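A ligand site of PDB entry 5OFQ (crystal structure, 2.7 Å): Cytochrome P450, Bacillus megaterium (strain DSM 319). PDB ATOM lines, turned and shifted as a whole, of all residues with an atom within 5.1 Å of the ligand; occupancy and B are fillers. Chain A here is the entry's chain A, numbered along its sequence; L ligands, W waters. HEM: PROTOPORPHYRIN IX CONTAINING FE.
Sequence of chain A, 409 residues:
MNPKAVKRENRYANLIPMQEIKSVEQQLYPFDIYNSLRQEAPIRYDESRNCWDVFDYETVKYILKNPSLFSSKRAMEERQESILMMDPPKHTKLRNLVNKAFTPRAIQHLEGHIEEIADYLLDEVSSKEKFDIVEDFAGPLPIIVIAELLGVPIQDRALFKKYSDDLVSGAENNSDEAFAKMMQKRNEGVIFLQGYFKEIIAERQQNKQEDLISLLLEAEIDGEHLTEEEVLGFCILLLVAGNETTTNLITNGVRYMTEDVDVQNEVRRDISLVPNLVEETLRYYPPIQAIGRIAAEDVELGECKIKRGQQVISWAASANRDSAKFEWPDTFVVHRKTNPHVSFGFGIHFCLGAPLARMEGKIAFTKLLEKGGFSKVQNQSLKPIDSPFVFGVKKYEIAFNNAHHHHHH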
ATOM      1  N   LEU A  64      25.213   9.002 -17.573  1.00  0.00           N
ATOM      2  CA  LEU A  64      25.219   9.709 -16.302  1.00  0.00           C
ATOM      3  C   LEU A  64      25.856  11.077 -16.427  1.00  0.00           C
ATOM      4  O   LEU A  64      25.493  12.014 -15.708  1.00  0.00           O
ATOM      5  CB  LEU A  64      25.938   8.879 -15.252  1.00  0.00           C
ATOM      6  CG  LEU A  64      25.405   7.460 -15.032  1.00  0.00           C
ATOM      7  CD1 LEU A  64      26.306   6.697 -14.138  1.00  0.00           C
ATOM      8  CD2 LEU A  64      24.036   7.455 -14.454  1.00  0.00           C
ATOM      9  N   SER A  72      16.936  12.790 -14.691  1.00  0.00           N
ATOM     10  CA  SER A  72      16.615  12.107 -13.439  1.00  0.00           C
ATOM     11  C   SER A  72      15.194  12.405 -12.978  1.00  0.00           C
ATOM     12  O   SER A  72      14.732  11.779 -12.013  1.00  0.00           O
ATOM     13  CB  SER A  72      17.627  12.515 -12.377  1.00  0.00           C
ATOM     14  OG  SER A  72      18.950  12.306 -12.811  1.00  0.00           O
ATOM     15  N   ILE A  83      16.746  15.289  -3.981  1.00  0.00           N
ATOM     16  CA  ILE A  83      17.648  15.628  -5.087  1.00  0.00           C
ATOM     17  C   ILE A  83      17.860  14.492  -6.070  1.00  0.00           C
ATOM     18  O   ILE A  83      18.209  14.747  -7.217  1.00  0.00           O
ATOM     19  CB  ILE A  83      19.005  16.099  -4.554  1.00  0.00           C
ATOM     20  CG1 ILE A  83      19.584  15.037  -3.645  1.00  0.00           C
ATOM     21  CG2 ILE A  83      18.785  17.414  -3.825  1.00  0.00           C
ATOM     22  CD1 ILE A  83      20.927  15.336  -3.142  1.00  0.00           C
ATOM     23  N   LEU A  84      17.681  13.249  -5.656  1.00  0.00           N
ATOM     24  CA  LEU A  84      17.849  12.137  -6.567  1.00  0.00           C
ATOM     25  C   LEU A  84      17.020  12.261  -7.852  1.00  0.00           C
ATOM     26  O   LEU A  84      17.459  11.794  -8.903  1.00  0.00           O
ATOM     27  CB  LEU A  84      17.479  10.877  -5.820  1.00  0.00           C
ATOM     28  CG  LEU A  84      17.481   9.572  -6.584  1.00  0.00           C
ATOM     29  CD1 LEU A  84      18.888   9.133  -6.888  1.00  0.00           C
ATOM     30  CD2 LEU A  84      16.684   8.579  -5.757  1.00  0.00           C
ATOM     31  N   HIS A  91      18.621  20.791  -9.225  1.00  0.00           N
ATOM     32  CA  HIS A  91      19.426  19.789  -8.533  1.00  0.00           C
ATOM     33  C   HIS A  91      20.720  20.368  -8.055  1.00  0.00           C
ATOM     34  O   HIS A  91      21.255  19.960  -7.031  1.00  0.00           O
ATOM     35  CB  HIS A  91      19.744  18.631  -9.463  1.00  0.00           C
ATOM     36  CG  HIS A  91      20.867  17.767  -8.977  1.00  0.00           C
ATOM     37  ND1 HIS A  91      22.197  18.047  -9.245  1.00  0.00           N
ATOM     38  CD2 HIS A  91      20.862  16.660  -8.206  1.00  0.00           C
ATOM     39  CE1 HIS A  91      22.953  17.130  -8.682  1.00  0.00           C
ATOM     40  NE2 HIS A  91      22.163  16.269  -8.055  1.00  0.00           N
ATOM     41  N   ARG A  95      21.710  20.181  -4.036  1.00  0.00           N
ATOM     42  CA  ARG A  95      22.929  19.444  -3.724  1.00  0.00           C
ATOM     43  C   ARG A  95      23.963  20.348  -3.088  1.00  0.00           C
ATOM     44  O   ARG A  95      24.570  19.976  -2.082  1.00  0.00           O
ATOM     45  CB  ARG A  95      23.474  18.770  -4.987  1.00  0.00           C
ATOM     46  CG  ARG A  95      24.849  18.143  -4.876  1.00  0.00           C
ATOM     47  CD  ARG A  95      24.663  16.748  -4.743  1.00  0.00           C
ATOM     48  NE  ARG A  95      25.902  16.026  -4.599  1.00  0.00           N
ATOM     49  CZ  ARG A  95      26.020  14.714  -4.806  1.00  0.00           C
ATOM     50  NH1 ARG A  95      24.974  13.983  -5.159  1.00  0.00           N
ATOM     51  NH2 ARG A  95      27.172  14.139  -4.631  1.00  0.00           N
ATOM     52  N   PHE A 102      28.793  15.966   3.806  1.00  0.00           N
ATOM     53  CA  PHE A 102      29.020  14.583   3.418  1.00  0.00           C
ATOM     54  C   PHE A 102      30.425  14.296   2.902  1.00  0.00           C
ATOM     55  O   PHE A 102      30.741  13.138   2.645  1.00  0.00           O
ATOM     56  CB  PHE A 102      27.945  14.183   2.415  1.00  0.00           C
ATOM     57  CG  PHE A 102      26.583  14.139   3.016  1.00  0.00           C
ATOM     58  CD1 PHE A 102      25.809  15.254   3.025  1.00  0.00           C
ATOM     59  CD2 PHE A 102      26.105  13.001   3.630  1.00  0.00           C
ATOM     60  CE1 PHE A 102      24.569  15.243   3.611  1.00  0.00           C
ATOM     61  CE2 PHE A 102      24.886  12.987   4.203  1.00  0.00           C
ATOM     62  CZ  PHE A 102      24.114  14.104   4.190  1.00  0.00           C
ATOM     63  N   ILE A 146      23.025   6.866  10.841  1.00  0.00           N
ATOM     64  CA  ILE A 146      22.298   7.971  10.248  1.00  0.00           C
ATOM     65  C   ILE A 146      21.373   8.596  11.291  1.00  0.00           C
ATOM     66  O   ILE A 146      20.989   9.760  11.174  1.00  0.00           O
ATOM     67  CB  ILE A 146      21.545   7.470   9.002  1.00  0.00           C
ATOM     68  CG1 ILE A 146      21.294   8.618   8.021  1.00  0.00           C
ATOM     69  CG2 ILE A 146      20.227   6.821   9.376  1.00  0.00           C
ATOM     70  CD1 ILE A 146      22.485   9.101   7.335  1.00  0.00           C
ATOM     71  N   PHE A 234      14.860  15.413   1.994  1.00  0.00           N
ATOM     72  CA  PHE A 234      16.240  14.968   1.973  1.00  0.00           C
ATOM     73  C   PHE A 234      16.498  13.970   3.089  1.00  0.00           C
ATOM     74  O   PHE A 234      17.218  13.001   2.895  1.00  0.00           O
ATOM     75  CB  PHE A 234      17.156  16.169   2.085  1.00  0.00           C
ATOM     76  CG  PHE A 234      18.629  15.856   1.919  1.00  0.00           C
ATOM     77  CD1 PHE A 234      19.166  15.574   0.697  1.00  0.00           C
ATOM     78  CD2 PHE A 234      19.485  15.873   3.010  1.00  0.00           C
ATOM     79  CE1 PHE A 234      20.488  15.295   0.552  1.00  0.00           C
ATOM     80  CE2 PHE A 234      20.818  15.601   2.871  1.00  0.00           C
ATOM     81  CZ  PHE A 234      21.324  15.306   1.650  1.00  0.00           C
ATOM     82  N   LEU A 237      15.136  10.807   1.934  1.00  0.00           N
ATOM     83  CA  LEU A 237      16.029  10.231   0.945  1.00  0.00           C
ATOM     84  C   LEU A 237      17.217   9.532   1.616  1.00  0.00           C
ATOM     85  O   LEU A 237      17.485   8.364   1.337  1.00  0.00           O
ATOM     86  CB  LEU A 237      16.496  11.299  -0.017  1.00  0.00           C
ATOM     87  CG  LEU A 237      17.442  10.889  -1.132  1.00  0.00           C
ATOM     88  CD1 LEU A 237      16.821   9.891  -2.022  1.00  0.00           C
ATOM     89  CD2 LEU A 237      17.862  12.093  -1.900  1.00  0.00           C
ATOM     90  N   LEU A 238      17.904  10.198   2.557  1.00  0.00           N
ATOM     91  CA  LEU A 238      19.056   9.575   3.204  1.00  0.00           C
ATOM     92  C   LEU A 238      18.724   8.193   3.754  1.00  0.00           C
ATOM     93  O   LEU A 238      19.602   7.322   3.830  1.00  0.00           O
ATOM     94  CB  LEU A 238      19.588  10.438   4.334  1.00  0.00           C
ATOM     95  CG  LEU A 238      20.102  11.809   3.912  1.00  0.00           C
ATOM     96  CD1 LEU A 238      20.671  12.640   5.073  1.00  0.00           C
ATOM     97  CD2 LEU A 238      21.113  11.608   2.845  1.00  0.00           C
ATOM     98  N   ALA A 241      18.074   6.073   0.404  1.00  0.00           N
ATOM     99  CA  ALA A 241      19.299   5.916  -0.365  1.00  0.00           C
ATOM    100  C   ALA A 241      20.411   5.284   0.441  1.00  0.00           C
ATOM    101  O   ALA A 241      21.298   4.657  -0.162  1.00  0.00           O
ATOM    102  CB  ALA A 241      19.799   7.267  -0.885  1.00  0.00           C
ATOM    103  N   GLY A 242      20.384   5.418   1.764  1.00  0.00           N
ATOM    104  CA  GLY A 242      21.549   5.162   2.581  1.00  0.00           C
ATOM    105  C   GLY A 242      21.575   3.907   3.413  1.00  0.00           C
ATOM    106  O   GLY A 242      22.655   3.461   3.846  1.00  0.00           O
ATOM    107  N   THR A 245      21.360   0.039   0.976  1.00  0.00           N
ATOM    108  CA  THR A 245      22.570  -0.046   0.170  1.00  0.00           C
ATOM    109  C   THR A 245      23.812  -0.316   1.009  1.00  0.00           C
ATOM    110  O   THR A 245      24.593  -1.204   0.693  1.00  0.00           O
ATOM    111  CB  THR A 245      22.711   1.254  -0.583  1.00  0.00           C
ATOM    112  OG1 THR A 245      22.569   2.306   0.363  1.00  0.00           O
ATOM    113  CG2 THR A 245      21.636   1.381  -1.622  1.00  0.00           C
ATOM    114  N   THR A 246      24.046   0.480   2.057  1.00  0.00           N
ATOM    115  CA  THR A 246      25.143   0.218   2.974  1.00  0.00           C
ATOM    116  C   THR A 246      25.028  -1.168   3.587  1.00  0.00           C
ATOM    117  O   THR A 246      25.973  -1.964   3.586  1.00  0.00           O
ATOM    118  CB  THR A 246      25.154   1.291   4.054  1.00  0.00           C
ATOM    119  OG1 THR A 246      25.157   2.562   3.415  1.00  0.00           O
ATOM    120  CG2 THR A 246      26.329   1.193   4.941  1.00  0.00           C
ATOM    121  N   LEU A 249      26.200  -3.357   1.066  1.00  0.00           N
ATOM    122  CA  LEU A 249      27.659  -3.333   0.988  1.00  0.00           C
ATOM    123  C   LEU A 249      28.275  -4.246   2.035  1.00  0.00           C
ATOM    124  O   LEU A 249      29.118  -5.073   1.716  1.00  0.00           O
ATOM    125  CB  LEU A 249      28.179  -1.921   1.158  1.00  0.00           C
ATOM    126  CG  LEU A 249      29.689  -1.797   1.439  1.00  0.00           C
ATOM    127  CD1 LEU A 249      30.549  -2.339   0.361  1.00  0.00           C
ATOM    128  CD2 LEU A 249      30.002  -0.381   1.546  1.00  0.00           C
ATOM    129  N   LEU A 282      32.118  -3.039  -3.871  1.00  0.00           N
ATOM    130  CA  LEU A 282      31.191  -2.213  -4.641  1.00  0.00           C
ATOM    131  C   LEU A 282      31.220  -2.553  -6.124  1.00  0.00           C
ATOM    132  O   LEU A 282      30.176  -2.586  -6.774  1.00  0.00           O
ATOM    133  CB  LEU A 282      31.501  -0.713  -4.443  1.00  0.00           C
ATOM    134  CG  LEU A 282      31.215  -0.151  -3.063  1.00  0.00           C
ATOM    135  CD1 LEU A 282      31.968   1.103  -2.870  1.00  0.00           C
ATOM    136  CD2 LEU A 282      29.732   0.137  -2.914  1.00  0.00           C
ATOM    137  N   PRO A 287      25.729  -2.942  -4.584  1.00  0.00           N
ATOM    138  CA  PRO A 287      24.401  -2.888  -3.988  1.00  0.00           C
ATOM    139  C   PRO A 287      23.344  -2.375  -4.939  1.00  0.00           C
ATOM    140  O   PRO A 287      22.204  -2.879  -4.947  1.00  0.00           O
ATOM    141  CB  PRO A 287      24.641  -1.964  -2.806  1.00  0.00           C
ATOM    142  CG  PRO A 287      26.014  -2.199  -2.438  1.00  0.00           C
ATOM    143  CD  PRO A 287      26.726  -2.357  -3.682  1.00  0.00           C
ATOM    144  N   ILE A 288      23.679  -1.402  -5.759  1.00  0.00           N
ATOM    145  CA  ILE A 288      22.724  -0.901  -6.745  1.00  0.00           C
ATOM    146  C   ILE A 288      23.192  -1.367  -8.106  1.00  0.00           C
ATOM    147  O   ILE A 288      24.192  -0.866  -8.604  1.00  0.00           O
ATOM    148  CB  ILE A 288      22.616   0.637  -6.737  1.00  0.00           C
ATOM    149  CG1 ILE A 288      22.111   1.182  -5.387  1.00  0.00           C
ATOM    150  CG2 ILE A 288      21.824   1.073  -7.969  1.00  0.00           C
ATOM    151  CD1 ILE A 288      20.889   0.608  -4.908  1.00  0.00           C
ATOM    152  N   ILE A 291      20.857   2.005 -12.755  1.00  0.00           N
ATOM    153  CA  ILE A 291      20.484   3.406 -12.595  1.00  0.00           C
ATOM    154  C   ILE A 291      19.480   3.728 -13.692  1.00  0.00           C
ATOM    155  O   ILE A 291      19.766   3.516 -14.876  1.00  0.00           O
ATOM    156  CB  ILE A 291      21.671   4.352 -12.784  1.00  0.00           C
ATOM    157  CG1 ILE A 291      22.936   3.828 -12.122  1.00  0.00           C
ATOM    158  CG2 ILE A 291      21.320   5.666 -12.199  1.00  0.00           C
ATOM    159  CD1 ILE A 291      22.975   3.986 -10.707  1.00  0.00           C
ATOM    160  N   GLY A 292      18.354   4.299 -13.314  1.00  0.00           N
ATOM    161  CA  GLY A 292      17.375   4.687 -14.293  1.00  0.00           C
ATOM    162  C   GLY A 292      17.541   6.131 -14.720  1.00  0.00           C
ATOM    163  O   GLY A 292      18.014   6.972 -13.957  1.00  0.00           O
ATOM    164  N   ARG A 293      17.196   6.395 -15.980  1.00  0.00           N
ATOM    165  CA  ARG A 293      17.074   7.738 -16.510  1.00  0.00           C
ATOM    166  C   ARG A 293      15.912   7.727 -17.503  1.00  0.00           C
ATOM    167  O   ARG A 293      15.537   6.683 -18.031  1.00  0.00           O
ATOM    168  CB  ARG A 293      18.384   8.172 -17.194  1.00  0.00           C
ATOM    169  CG  ARG A 293      19.589   8.381 -16.282  1.00  0.00           C
ATOM    170  CD  ARG A 293      19.546   9.690 -15.507  1.00  0.00           C
ATOM    171  NE  ARG A 293      20.729   9.958 -14.702  1.00  0.00           N
ATOM    172  CZ  ARG A 293      20.899   9.572 -13.442  1.00  0.00           C
ATOM    173  NH1 ARG A 293      19.994   8.884 -12.806  1.00  0.00           N
ATOM    174  NH2 ARG A 293      21.994   9.886 -12.818  1.00  0.00           N
ATOM    175  N   VAL A 342      31.147   2.440 -11.123  1.00  0.00           N
ATOM    176  CA  VAL A 342      30.004   3.326 -11.115  1.00  0.00           C
ATOM    177  C   VAL A 342      28.964   2.792 -10.150  1.00  0.00           C
ATOM    178  O   VAL A 342      27.760   3.008 -10.325  1.00  0.00           O
ATOM    179  CB  VAL A 342      29.404   3.463 -12.528  1.00  0.00           C
ATOM    180  CG1 VAL A 342      30.374   4.231 -13.357  1.00  0.00           C
ATOM    181  CG2 VAL A 342      29.165   2.070 -13.178  1.00  0.00           C
ATOM    182  N   SER A 343      29.428   2.100  -9.114  1.00  0.00           N
ATOM    183  CA  SER A 343      28.546   1.633  -8.067  1.00  0.00           C
ATOM    184  C   SER A 343      27.966   2.797  -7.276  1.00  0.00           C
ATOM    185  O   SER A 343      26.938   2.625  -6.624  1.00  0.00           O
ATOM    186  CB  SER A 343      29.309   0.703  -7.139  1.00  0.00           C
ATOM    187  OG  SER A 343      29.721  -0.449  -7.804  1.00  0.00           O
ATOM    188  N   PHE A 344      28.625   3.951  -7.241  1.00  0.00           N
ATOM    189  CA  PHE A 344      28.040   5.159  -6.661  1.00  0.00           C
ATOM    190  C   PHE A 344      27.526   6.116  -7.719  1.00  0.00           C
ATOM    191  O   PHE A 344      27.339   7.281  -7.435  1.00  0.00           O
ATOM    192  CB  PHE A 344      29.053   5.877  -5.779  1.00  0.00           C
ATOM    193  CG  PHE A 344      29.352   5.192  -4.500  1.00  0.00           C
ATOM    194  CD1 PHE A 344      28.355   4.925  -3.595  1.00  0.00           C
ATOM    195  CD2 PHE A 344      30.644   4.851  -4.172  1.00  0.00           C
ATOM    196  CE1 PHE A 344      28.623   4.307  -2.419  1.00  0.00           C
ATOM    197  CE2 PHE A 344      30.919   4.231  -2.973  1.00  0.00           C
ATOM    198  CZ  PHE A 344      29.884   3.959  -2.098  1.00  0.00           C
ATOM    199  N   GLY A 345      27.385   5.663  -8.942  1.00  0.00           N
ATOM    200  CA  GLY A 345      26.991   6.497 -10.046  1.00  0.00           C
ATOM    201  C   GLY A 345      28.185   7.196 -10.661  1.00  0.00           C
ATOM    202  O   GLY A 345      29.326   6.771 -10.533  1.00  0.00           O
ATOM    203  N   ILE A 348      26.947  14.362 -11.624  1.00  0.00           N
ATOM    204  CA  ILE A 348      26.352  15.308 -10.702  1.00  0.00           C
ATOM    205  C   ILE A 348      25.501  14.601  -9.655  1.00  0.00           C
ATOM    206  O   ILE A 348      25.295  15.153  -8.587  1.00  0.00           O
ATOM    207  CB  ILE A 348      25.521  16.377 -11.424  1.00  0.00           C
ATOM    208  CG1 ILE A 348      24.330  15.735 -12.151  1.00  0.00           C
ATOM    209  CG2 ILE A 348      26.379  17.148 -12.404  1.00  0.00           C
ATOM    210  CD1 ILE A 348      23.370  16.721 -12.783  1.00  0.00           C
ATOM    211  N   HIS A 349      25.014  13.387  -9.908  1.00  0.00           N
ATOM    212  CA  HIS A 349      24.207  12.689  -8.911  1.00  0.00           C
ATOM    213  C   HIS A 349      25.036  11.679  -8.114  1.00  0.00           C
ATOM    214  O   HIS A 349      24.463  10.861  -7.405  1.00  0.00           O
ATOM    215  CB  HIS A 349      23.019  11.962  -9.562  1.00  0.00           C
ATOM    216  CG  HIS A 349      21.962  12.882 -10.113  1.00  0.00           C
ATOM    217  ND1 HIS A 349      20.920  13.373  -9.360  1.00  0.00           N
ATOM    218  CD2 HIS A 349      21.775  13.380 -11.362  1.00  0.00           C
ATOM    219  CE1 HIS A 349      20.150  14.130 -10.115  1.00  0.00           C
ATOM    220  NE2 HIS A 349      20.657  14.160 -11.338  1.00  0.00           N
ATOM    221  N   PHE A 350      26.369  11.718  -8.253  1.00  0.00           N
ATOM    222  CA  PHE A 350      27.269  10.760  -7.608  1.00  0.00           C
ATOM    223  C   PHE A 350      27.004  10.695  -6.112  1.00  0.00           C
ATOM    224  O   PHE A 350      26.977  11.709  -5.434  1.00  0.00           O
ATOM    225  CB  PHE A 350      28.749  11.126  -7.842  1.00  0.00           C
ATOM    226  CG  PHE A 350      29.722  10.146  -7.254  1.00  0.00           C
ATOM    227  CD1 PHE A 350      30.148   9.043  -7.958  1.00  0.00           C
ATOM    228  CD2 PHE A 350      30.213  10.328  -6.000  1.00  0.00           C
ATOM    229  CE1 PHE A 350      31.046   8.137  -7.411  1.00  0.00           C
ATOM    230  CE2 PHE A 350      31.081   9.429  -5.463  1.00  0.00           C
ATOM    231  CZ  PHE A 350      31.498   8.332  -6.176  1.00  0.00           C
ATOM    232  N   CYS A 351      26.812   9.482  -5.619  1.00  0.00           N
ATOM    233  CA  CYS A 351      26.321   9.283  -4.267  1.00  0.00           C
ATOM    234  C   CYS A 351      26.900  10.316  -3.321  1.00  0.00           C
ATOM    235  O   CYS A 351      28.115  10.419  -3.139  1.00  0.00           O
ATOM    236  CB  CYS A 351      26.653   7.897  -3.760  1.00  0.00           C
ATOM    237  SG  CYS A 351      25.758   7.490  -2.314  1.00  0.00           S
ATOM    238  N   LEU A 352      26.000  11.088  -2.755  1.00  0.00           N
ATOM    239  CA  LEU A 352      26.377  11.986  -1.699  1.00  0.00           C
ATOM    240  C   LEU A 352      26.878  11.228  -0.488  1.00  0.00           C
ATOM    241  O   LEU A 352      27.588  11.789   0.338  1.00  0.00           O
ATOM    242  CB  LEU A 352      25.194  12.870  -1.360  1.00  0.00           C
ATOM    243  CG  LEU A 352      25.410  13.971  -0.339  1.00  0.00           C
ATOM    244  CD1 LEU A 352      26.359  15.105  -0.797  1.00  0.00           C
ATOM    245  CD2 LEU A 352      23.973  14.475  -0.008  1.00  0.00           C
ATOM    246  N   GLY A 353      26.516   9.947  -0.366  1.00  0.00           N
ATOM    247  CA  GLY A 353      26.828   9.176   0.808  1.00  0.00           C
ATOM    248  C   GLY A 353      28.008   8.251   0.659  1.00  0.00           C
ATOM    249  O   GLY A 353      28.226   7.418   1.544  1.00  0.00           O
ATOM    250  N   ALA A 354      28.780   8.387  -0.412  1.00  0.00           N
ATOM    251  CA  ALA A 354      29.937   7.521  -0.633  1.00  0.00           C
ATOM    252  C   ALA A 354      30.987   7.645   0.461  1.00  0.00           C
ATOM    253  O   ALA A 354      31.516   6.602   0.886  1.00  0.00           O
ATOM    254  CB  ALA A 354      30.522   7.806  -2.005  1.00  0.00           C
ATOM    255  N   LEU A 356      30.447   8.357   3.611  1.00  0.00           N
ATOM    256  CA  LEU A 356      29.853   7.686   4.751  1.00  0.00           C
ATOM    257  C   LEU A 356      29.735   6.176   4.515  1.00  0.00           C
ATOM    258  O   LEU A 356      30.095   5.376   5.386  1.00  0.00           O
ATOM    259  CB  LEU A 356      28.502   8.319   5.068  1.00  0.00           C
ATOM    260  CG  LEU A 356      27.768   7.775   6.268  1.00  0.00           C
ATOM    261  CD1 LEU A 356      28.638   7.911   7.524  1.00  0.00           C
ATOM    262  CD2 LEU A 356      26.463   8.504   6.387  1.00  0.00           C
ATOM    263  N   ALA A 357      29.230   5.770   3.364  1.00  0.00           N
ATOM    264  CA  ALA A 357      29.161   4.350   3.046  1.00  0.00           C
ATOM    265  C   ALA A 357      30.562   3.724   3.063  1.00  0.00           C
ATOM    266  O   ALA A 357      30.760   2.640   3.638  1.00  0.00           O
ATOM    267  CB  ALA A 357      28.495   4.132   1.681  1.00  0.00           C
HETATM  268  CHA HEM L   1      22.812   8.678  -4.925  1.00  0.00           C
HETATM  269  CHB HEM L   1      24.421   4.241  -4.557  1.00  0.00           C
HETATM  270  CHC HEM L   1      24.950   4.806   0.207  1.00  0.00           C
HETATM  271  CHD HEM L   1      22.885   9.017  -0.204  1.00  0.00           C
HETATM  272  C1A HEM L   1      23.291   7.444  -5.266  1.00  0.00           C
HETATM  273  C2A HEM L   1      23.477   6.944  -6.613  1.00  0.00           C
HETATM  274  C3A HEM L   1      23.909   5.727  -6.490  1.00  0.00           C
HETATM  275  C4A HEM L   1      24.003   5.416  -5.090  1.00  0.00           C
HETATM  276  CMA HEM L   1      24.251   4.828  -7.666  1.00  0.00           C
HETATM  277  CAA HEM L   1      23.244   7.687  -7.943  1.00  0.00           C
HETATM  278  CBA HEM L   1      21.895   7.332  -8.543  1.00  0.00           C
HETATM  279  CGA HEM L   1      21.547   8.146  -9.764  1.00  0.00           C
HETATM  280  O1A HEM L   1      22.523   8.632 -10.383  1.00  0.00           O
HETATM  281  O2A HEM L   1      20.340   8.331 -10.092  1.00  0.00           O
HETATM  282  C1B HEM L   1      24.744   4.033  -3.238  1.00  0.00           C
HETATM  283  C2B HEM L   1      25.422   2.877  -2.695  1.00  0.00           C
HETATM  284  C3B HEM L   1      25.538   3.045  -1.385  1.00  0.00           C
HETATM  285  C4B HEM L   1      24.961   4.315  -1.065  1.00  0.00           C
HETATM  286  CMB HEM L   1      25.901   1.655  -3.508  1.00  0.00           C
HETATM  287  CAB HEM L   1      26.215   2.176  -0.316  1.00  0.00           C
HETATM  288  CBB HEM L   1      27.164   1.276  -0.613  1.00  0.00           C
HETATM  289  C1C HEM L   1      24.431   6.008   0.523  1.00  0.00           C
HETATM  290  C2C HEM L   1      24.411   6.569   1.816  1.00  0.00           C
HETATM  291  C3C HEM L   1      23.825   7.732   1.718  1.00  0.00           C
HETATM  292  C4C HEM L   1      23.496   7.918   0.324  1.00  0.00           C
HETATM  293  CMC HEM L   1      24.983   5.874   3.039  1.00  0.00           C
HETATM  294  CAC HEM L   1      23.531   8.755   2.835  1.00  0.00           C
HETATM  295  CBC HEM L   1      23.430   8.408   4.123  1.00  0.00           C
HETATM  296  C1D HEM L   1      22.663   9.288  -1.509  1.00  0.00           C
HETATM  297  C2D HEM L   1      22.005  10.461  -2.040  1.00  0.00           C
HETATM  298  C3D HEM L   1      21.970  10.348  -3.342  1.00  0.00           C
HETATM  299  C4D HEM L   1      22.619   9.117  -3.667  1.00  0.00           C
HETATM  300  CMD HEM L   1      21.424  11.628  -1.235  1.00  0.00           C
HETATM  301  CAD HEM L   1      21.364  11.359  -4.335  1.00  0.00           C
HETATM  302  CBD HEM L   1      22.461  12.251  -4.880  1.00  0.00           C
HETATM  303  CGD HEM L   1      21.885  13.046  -6.001  1.00  0.00           C
HETATM  304  O1D HEM L   1      22.493  14.092  -6.329  1.00  0.00           O
HETATM  305  O2D HEM L   1      20.842  12.636  -6.551  1.00  0.00           O
HETATM  306  NA  HEM L   1      23.613   6.490  -4.342  1.00  0.00           N
HETATM  307  NB  HEM L   1      24.460   4.908  -2.205  1.00  0.00           N
HETATM  308  NC  HEM L   1      23.884   6.828  -0.399  1.00  0.00           N
HETATM  309  ND  HEM L   1      23.040   8.472  -2.556  1.00  0.00           N
HETATM  310 FE   HEM L   1      23.693   6.576  -2.490  1.00  0.00          FE
HETATM  311  O   HOH W   1      26.279   0.108  -6.610  1.00  0.00           O
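ND1 of His 349 lies within hydrogen-bond range of O2D of the ligand (2.9 Å). NH2 of Arg 293 is in salt-bridge range of O1A of the ligand. NE2 of His 91 lies within hydrogen-bond range of O1D of the ligand. An oxygen (O2D) of the ligand sits close to the backbone NH (N) of Leu 84, at 3.3 Å. The side-chain sulfur (SG) of Cys 351 binds an iron atom (FE) of the ligand, at 2.3 Å. NH1 of Arg 95 is in salt-bridge range of O1D of the ligand, at 2.7 Å.
The side-chain sulfur (SG) of Cys 351 sits close to the backbone NH (N) of Ala 354 (3.7 Å). The guanidinium group of Arg 95 lies within hydrogen-bond range of the backbone carbonyl oxygen of Phe 350, 2.6 Å away. The backbone carbonyl oxygen (O) of Ala 241 sits at hydrogen-bond distance from the side-chain hydroxyl (OG1) of Thr 245 (2.7 Å). NE2 of His 91 sits at hydrogen-bond distance from ND1 of His 349 (3.4 Å). The side-chain hydroxyl (OG1) of Thr 246 is in hydrogen-bond range of the backbone carbonyl oxygen (O) of Gly 242, 2.7 Å away. OG of Ser 72 sits at hydrogen-bond distance from NE2 of His 349 (2.9 Å). The side-chain sulfur (SG) of Cys 351 sits close to the backbone NH (N) of Gly 353 (3.2 Å). The backbone carbonyl oxygen (O) of Phe 344 is in hydrogen-bond range of the backbone NH (N) of Cys 351, 2.9 Å away.
O of Ile 83 lies close to O2D of the ligand. A nitrogen (NC) of the ligand lies close to the backbone carbonyl oxygen (O) of Ala 241, at 3.4 Å. Residues that only touch the ligand: Ile 146 (3.4 Å), Leu 237 (3.7 Å), Leu 238 (3.7 Å), Gly 242 (3.3 Å), Thr 245 (3.4 Å), Thr 246 (3.3 Å), Leu 249 (3.8 Å), Leu 282 (3.6 Å), Pro 287 (3.9 Å), Ile 288 (3.9 Å), Ile 291 (3.4 Å), Ser 343 (3.4 Å), Phe 344 (3.5 Å), Gly 345 (3.5 Å), Ile 348 (3.8 Å), Leu 352 (3.96 Å), Gly 353 (3.5 Å), Leu 356 (3.8 Å) and Ala 357 (3.6 Å). Hydrophobic or aromatic side chains within 4 Å of the ligand: Ile 83, Leu 84, His 91, Ile 146, Leu 237, Leu 238, Ala 241, Leu 249, Leu 282, Pro 287, Ile 288, Ile 291, Phe 344, His 349, Leu 352, Leu 356 and Ala 357. 27 residues have an atom within 4 Å of the ligand: Ile 83, Leu 84, His 91, Arg 95, Ile 146, Leu 237, Leu 238, Ala 241, Gly 242, Thr 245, Thr 246, Leu 249, Leu 282, Pro 287, Ile 288, Ile 291, Arg 293, Ser 343, Phe 344, Gly 345, Ile 348, His 349, Cys 351, Leu 352, Gly 353, Leu 356 and Ala 357.
Water W1 bridges the backbone carbonyl oxygen of Ser 343 (2.6 Å) and the backbone carbonyl oxygen of Ile 288 (3.0 Å).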
